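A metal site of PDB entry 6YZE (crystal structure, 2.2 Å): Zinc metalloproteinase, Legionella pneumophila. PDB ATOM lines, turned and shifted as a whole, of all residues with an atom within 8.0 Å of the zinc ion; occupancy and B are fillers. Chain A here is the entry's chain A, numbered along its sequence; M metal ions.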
ATOM      1  N   ALA A 143      10.258 -15.489  21.539  1.00  0.00           N
ATOM      2  CA  ALA A 143       9.287 -15.265  20.491  1.00  0.00           C
ATOM      3  C   ALA A 143      10.062 -15.165  19.198  1.00  0.00           C
ATOM      4  O   ALA A 143      11.151 -14.583  19.185  1.00  0.00           O
ATOM      5  CB  ALA A 143       8.464 -13.997  20.720  1.00  0.00           C
ATOM      6  N   TYR A 144       9.542 -15.739  18.106  1.00  0.00           N
ATOM      7  CA  TYR A 144      10.376 -15.829  16.911  1.00  0.00           C
ATOM      8  C   TYR A 144       9.554 -15.721  15.625  1.00  0.00           C
ATOM      9  O   TYR A 144       8.347 -15.988  15.598  1.00  0.00           O
ATOM     10  CB  TYR A 144      11.212 -17.108  16.906  1.00  0.00           C
ATOM     11  CG  TYR A 144      10.436 -18.402  16.701  1.00  0.00           C
ATOM     12  CD1 TYR A 144      10.135 -18.855  15.426  1.00  0.00           C
ATOM     13  CD2 TYR A 144      10.055 -19.187  17.789  1.00  0.00           C
ATOM     14  CE1 TYR A 144       9.453 -20.044  15.241  1.00  0.00           C
ATOM     15  CE2 TYR A 144       9.390 -20.389  17.611  1.00  0.00           C
ATOM     16  CZ  TYR A 144       9.085 -20.801  16.334  1.00  0.00           C
ATOM     17  OH  TYR A 144       8.401 -21.989  16.127  1.00  0.00           O
ATOM     18  N   TRP A 145      10.259 -15.349  14.559  1.00  0.00           N
ATOM     19  CA  TRP A 145       9.737 -15.243  13.203  1.00  0.00           C
ATOM     20  C   TRP A 145      10.248 -16.429  12.403  1.00  0.00           C
ATOM     21  O   TRP A 145      11.418 -16.782  12.517  1.00  0.00           O
ATOM     22  CB  TRP A 145      10.206 -13.923  12.557  1.00  0.00           C
ATOM     23  CG  TRP A 145      10.071 -13.822  11.060  1.00  0.00           C
ATOM     24  CD1 TRP A 145      11.085 -13.790  10.144  1.00  0.00           C
ATOM     25  CD2 TRP A 145       8.856 -13.710  10.312  1.00  0.00           C
ATOM     26  NE1 TRP A 145      10.576 -13.677   8.872  1.00  0.00           N
ATOM     27  CE2 TRP A 145       9.206 -13.626   8.950  1.00  0.00           C
ATOM     28  CE3 TRP A 145       7.508 -13.685  10.652  1.00  0.00           C
ATOM     29  CZ2 TRP A 145       8.268 -13.511   7.950  1.00  0.00           C
ATOM     30  CZ3 TRP A 145       6.574 -13.562   9.656  1.00  0.00           C
ATOM     31  CH2 TRP A 145       6.958 -13.484   8.318  1.00  0.00           C
ATOM     32  N   VAL A 167       7.963  -6.483  21.377  1.00  0.00           N
ATOM     33  CA  VAL A 167       8.353  -7.809  20.899  1.00  0.00           C
ATOM     34  C   VAL A 167       7.692  -8.112  19.560  1.00  0.00           C
ATOM     35  O   VAL A 167       8.350  -8.566  18.619  1.00  0.00           O
ATOM     36  CB  VAL A 167       7.989  -8.886  21.947  1.00  0.00           C
ATOM     37  CG1 VAL A 167       8.218 -10.269  21.363  1.00  0.00           C
ATOM     38  CG2 VAL A 167       8.807  -8.683  23.227  1.00  0.00           C
ATOM     39  N   HIS A 170       9.242  -6.086  16.839  1.00  0.00           N
ATOM     40  CA  HIS A 170      10.572  -6.645  16.600  1.00  0.00           C
ATOM     41  C   HIS A 170      10.502  -7.835  15.676  1.00  0.00           C
ATOM     42  O   HIS A 170      11.054  -7.815  14.565  1.00  0.00           O
ATOM     43  CB  HIS A 170      11.210  -7.049  17.925  1.00  0.00           C
ATOM     44  CG  HIS A 170      12.618  -7.533  17.769  1.00  0.00           C
ATOM     45  ND1 HIS A 170      13.707  -6.715  17.961  1.00  0.00           N
ATOM     46  CD2 HIS A 170      13.109  -8.740  17.410  1.00  0.00           C
ATOM     47  CE1 HIS A 170      14.813  -7.409  17.739  1.00  0.00           C
ATOM     48  NE2 HIS A 170      14.470  -8.636  17.402  1.00  0.00           N
ATOM     49  N   GLU A 171       9.816  -8.890  16.108  1.00  0.00           N
ATOM     50  CA  GLU A 171       9.840 -10.141  15.355  1.00  0.00           C
ATOM     51  C   GLU A 171       9.152 -10.008  13.995  1.00  0.00           C
ATOM     52  O   GLU A 171       9.677 -10.494  12.988  1.00  0.00           O
ATOM     53  CB  GLU A 171       9.192 -11.251  16.195  1.00  0.00           C
ATOM     54  CG  GLU A 171      10.084 -11.864  17.301  1.00  0.00           C
ATOM     55  CD  GLU A 171      11.484 -12.278  16.840  1.00  0.00           C
ATOM     56  OE1 GLU A 171      11.667 -12.668  15.674  1.00  0.00           O
ATOM     57  OE2 GLU A 171      12.416 -12.204  17.655  1.00  0.00           O
ATOM     58  N   VAL A 172       7.994  -9.353  13.940  1.00  0.00           N
ATOM     59  CA  VAL A 172       7.322  -9.156  12.649  1.00  0.00           C
ATOM     60  C   VAL A 172       8.272  -8.483  11.656  1.00  0.00           C
ATOM     61  O   VAL A 172       8.287  -8.822  10.466  1.00  0.00           O
ATOM     62  CB  VAL A 172       6.025  -8.335  12.826  1.00  0.00           C
ATOM     63  CG1 VAL A 172       5.451  -7.930  11.486  1.00  0.00           C
ATOM     64  CG2 VAL A 172       5.006  -9.123  13.602  1.00  0.00           C
ATOM     65  N   SER A 173       9.046  -7.504  12.093  1.00  0.00           N
ATOM     66  CA  SER A 173       9.793  -6.725  11.122  1.00  0.00           C
ATOM     67  C   SER A 173      10.998  -7.477  10.585  1.00  0.00           C
ATOM     68  O   SER A 173      11.634  -6.997   9.637  1.00  0.00           O
ATOM     69  CB  SER A 173      10.228  -5.400  11.750  1.00  0.00           C
ATOM     70  OG  SER A 173       9.101  -4.629  12.055  1.00  0.00           O
ATOM     71  N   HIS A 174      11.351  -8.623  11.176  1.00  0.00           N
ATOM     72  CA  HIS A 174      12.214  -9.574  10.484  1.00  0.00           C
ATOM     73  C   HIS A 174      11.580 -10.077   9.201  1.00  0.00           C
ATOM     74  O   HIS A 174      12.275 -10.450   8.262  1.00  0.00           O
ATOM     75  CB  HIS A 174      12.556 -10.738  11.394  1.00  0.00           C
ATOM     76  CG  HIS A 174      13.582 -10.418  12.419  1.00  0.00           C
ATOM     77  ND1 HIS A 174      14.834  -9.971  12.080  1.00  0.00           N
ATOM     78  CD2 HIS A 174      13.557 -10.511  13.766  1.00  0.00           C
ATOM     79  CE1 HIS A 174      15.535  -9.785  13.191  1.00  0.00           C
ATOM     80  NE2 HIS A 174      14.789 -10.113  14.218  1.00  0.00           N
ATOM     81  N   TYR A 185      21.654 -12.402   8.254  1.00  0.00           N
ATOM     82  CA  TYR A 185      21.636 -12.511   9.707  1.00  0.00           C
ATOM     83  C   TYR A 185      22.992 -12.944  10.267  1.00  0.00           C
ATOM     84  O   TYR A 185      23.117 -13.926  10.999  1.00  0.00           O
ATOM     85  CB  TYR A 185      20.535 -13.475  10.119  1.00  0.00           C
ATOM     86  CG  TYR A 185      20.004 -13.206  11.499  1.00  0.00           C
ATOM     87  CD1 TYR A 185      19.155 -12.143  11.730  1.00  0.00           C
ATOM     88  CD2 TYR A 185      20.332 -14.023  12.547  1.00  0.00           C
ATOM     89  CE1 TYR A 185      18.639 -11.908  13.003  1.00  0.00           C
ATOM     90  CE2 TYR A 185      19.831 -13.800  13.804  1.00  0.00           C
ATOM     91  CZ  TYR A 185      18.988 -12.744  14.020  1.00  0.00           C
ATOM     92  OH  TYR A 185      18.510 -12.540  15.269  1.00  0.00           O
ATOM     93  N   GLY A 190      23.875  -8.367   9.827  1.00  0.00           N
ATOM     94  CA  GLY A 190      23.081  -9.042  10.836  1.00  0.00           C
ATOM     95  C   GLY A 190      22.794  -8.153  12.027  1.00  0.00           C
ATOM     96  O   GLY A 190      21.711  -8.225  12.618  1.00  0.00           O
ATOM     97  N   ASN A 193      20.180  -5.845  10.729  1.00  0.00           N
ATOM     98  CA  ASN A 193      18.912  -6.556  10.755  1.00  0.00           C
ATOM     99  C   ASN A 193      18.326  -6.514  12.157  1.00  0.00           C
ATOM    100  O   ASN A 193      17.264  -5.943  12.375  1.00  0.00           O
ATOM    101  CB  ASN A 193      19.117  -7.999  10.274  1.00  0.00           C
ATOM    102  CG  ASN A 193      17.811  -8.773  10.137  1.00  0.00           C
ATOM    103  OD1 ASN A 193      16.962  -8.752  11.032  1.00  0.00           O
ATOM    104  ND2 ASN A 193      17.655  -9.488   9.023  1.00  0.00           N
ATOM    105  N   GLU A 194      19.031  -7.107  13.116  1.00  0.00           N
ATOM    106  CA  GLU A 194      18.607  -7.050  14.521  1.00  0.00           C
ATOM    107  C   GLU A 194      18.235  -5.617  14.933  1.00  0.00           C
ATOM    108  O   GLU A 194      17.218  -5.417  15.608  1.00  0.00           O
ATOM    109  CB  GLU A 194      19.715  -7.613  15.416  1.00  0.00           C
ATOM    110  CG  GLU A 194      19.415  -9.003  15.987  1.00  0.00           C
ATOM    111  CD  GLU A 194      17.942  -9.168  16.371  1.00  0.00           C
ATOM    112  OE1 GLU A 194      17.206  -9.864  15.657  1.00  0.00           O
ATOM    113  OE2 GLU A 194      17.512  -8.598  17.388  1.00  0.00           O
ATOM    114  N   SER A 195      19.023  -4.629  14.499  1.00  0.00           N
ATOM    115  CA  SER A 195      18.757  -3.234  14.835  1.00  0.00           C
ATOM    116  C   SER A 195      17.405  -2.769  14.282  1.00  0.00           C
ATOM    117  O   SER A 195      16.596  -2.173  15.008  1.00  0.00           O
ATOM    118  CB  SER A 195      19.871  -2.347  14.282  1.00  0.00           C
ATOM    119  OG  SER A 195      21.031  -2.406  15.097  1.00  0.00           O
ATOM    120  N   PHE A 196      17.168  -3.000  12.983  1.00  0.00           N
ATOM    121  CA  PHE A 196      15.916  -2.569  12.378  1.00  0.00           C
ATOM    122  C   PHE A 196      14.727  -3.060  13.190  1.00  0.00           C
ATOM    123  O   PHE A 196      13.782  -2.307  13.427  1.00  0.00           O
ATOM    124  CB  PHE A 196      15.811  -3.054  10.937  1.00  0.00           C
ATOM    125  CG  PHE A 196      14.581  -2.542  10.217  1.00  0.00           C
ATOM    126  CD1 PHE A 196      14.587  -1.302   9.602  1.00  0.00           C
ATOM    127  CD2 PHE A 196      13.416  -3.285  10.204  1.00  0.00           C
ATOM    128  CE1 PHE A 196      13.460  -0.830   8.964  1.00  0.00           C
ATOM    129  CE2 PHE A 196      12.288  -2.812   9.566  1.00  0.00           C
ATOM    130  CZ  PHE A 196      12.308  -1.588   8.944  1.00  0.00           C
ATOM    131  N   SER A 197      14.778  -4.322  13.640  1.00  0.00           N
ATOM    132  CA  SER A 197      13.670  -4.824  14.444  1.00  0.00           C
ATOM    133  C   SER A 197      13.553  -4.064  15.767  1.00  0.00           C
ATOM    134  O   SER A 197      12.435  -3.838  16.251  1.00  0.00           O
ATOM    135  CB  SER A 197      13.853  -6.318  14.672  1.00  0.00           C
ATOM    136  OG  SER A 197      13.900  -7.014  13.432  1.00  0.00           O
ATOM    137  N   ASP A 198      14.672  -3.633  16.349  1.00  0.00           N
ATOM    138  CA  ASP A 198      14.563  -2.880  17.590  1.00  0.00           C
ATOM    139  C   ASP A 198      13.989  -1.489  17.344  1.00  0.00           C
ATOM    140  O   ASP A 198      13.282  -0.947  18.201  1.00  0.00           O
ATOM    141  CB  ASP A 198      15.931  -2.810  18.282  1.00  0.00           C
ATOM    142  CG  ASP A 198      16.293  -4.091  18.984  1.00  0.00           C
ATOM    143  OD1 ASP A 198      15.374  -4.757  19.506  1.00  0.00           O
ATOM    144  OD2 ASP A 198      17.485  -4.467  19.010  1.00  0.00           O
ATOM    145  N   ARG A 231      17.870  -4.776  26.148  1.00  0.00           N
ATOM    146  CA  ARG A 231      18.792  -3.835  25.545  1.00  0.00           C
ATOM    147  C   ARG A 231      18.360  -2.403  25.836  1.00  0.00           C
ATOM    148  O   ARG A 231      17.172  -2.103  26.022  1.00  0.00           O
ATOM    149  CB  ARG A 231      18.883  -4.038  24.036  1.00  0.00           C
ATOM    150  CG  ARG A 231      19.481  -5.378  23.677  1.00  0.00           C
ATOM    151  CD  ARG A 231      19.593  -5.542  22.191  1.00  0.00           C
ATOM    152  NE  ARG A 231      18.339  -5.905  21.528  1.00  0.00           N
ATOM    153  CZ  ARG A 231      17.743  -7.086  21.641  1.00  0.00           C
ATOM    154  NH1 ARG A 231      18.250  -8.042  22.419  1.00  0.00           N
ATOM    155  NH2 ARG A 231      16.637  -7.310  20.955  1.00  0.00           N
ATOM    156  N   VAL A 255      24.638 -10.975  16.719  1.00  0.00           N
ATOM    157  CA  VAL A 255      23.896  -9.897  16.094  1.00  0.00           C
ATOM    158  C   VAL A 255      23.137  -9.085  17.146  1.00  0.00           C
ATOM    159  O   VAL A 255      22.957  -7.869  16.975  1.00  0.00           O
ATOM    160  CB  VAL A 255      22.975 -10.480  15.010  1.00  0.00           C
ATOM    161  CG1 VAL A 255      23.807 -11.028  13.856  1.00  0.00           C
ATOM    162  CG2 VAL A 255      22.092 -11.576  15.603  1.00  0.00           C
ATOM    163  N   HIS A 256      22.720  -9.712  18.256  1.00  0.00           N
ATOM    164  CA  HIS A 256      22.056  -8.993  19.337  1.00  0.00           C
ATOM    165  C   HIS A 256      22.987  -8.053  20.112  1.00  0.00           C
ATOM    166  O   HIS A 256      22.520  -7.425  21.064  1.00  0.00           O
ATOM    167  CB  HIS A 256      21.405  -9.977  20.312  1.00  0.00           C
ATOM    168  CG  HIS A 256      20.406 -10.879  19.664  1.00  0.00           C
ATOM    169  ND1 HIS A 256      20.659 -12.207  19.419  1.00  0.00           N
ATOM    170  CD2 HIS A 256      19.175 -10.628  19.170  1.00  0.00           C
ATOM    171  CE1 HIS A 256      19.598 -12.753  18.828  1.00  0.00           C
ATOM    172  NE2 HIS A 256      18.688 -11.810  18.670  1.00  0.00           N
HETATM  173 ZN    ZN M   1      15.488 -10.307  16.321  1.00  0.00          ZN
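OE2 of Glu 171 touches the zinc ion (3.8 Å). OH of Tyr 185 touches the zinc ion, at 3.9 Å.
The zinc ion is bound by OE1 of Glu 194, NE2 of His 174 and NE2 of His 170. The zinc ion has three donor atoms within binding distance.
The backbone carbonyl oxygen of His 170 sits at hydrogen-bond distance from the side-chain hydroxyl of Ser 197 (3.2 Å). OG of Ser 197 sits close to ND1 of His 174. ND1 of His 174 lies within hydrogen-bond range of OD1 of Asn 193 (2.7 Å). OE1 of Glu 171 is in hydrogen-bond range of N of Trp 145, at 3.2 Å. The side-chain carboxylate (OE2) of Glu 194 is in salt-bridge range of the guanidinium group (NH2) of Arg 231 (3.9 Å). The side-chain hydroxyl (OH) of Tyr 185 sits at hydrogen-bond distance from a ring nitrogen (NE2) of His 256, 3.5 Å away. OD1 of Asp 198 sits at hydrogen-bond distance from ND1 of His 170 (3.0 Å). OH of Tyr 185 sits close to OE1 of Glu 194.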
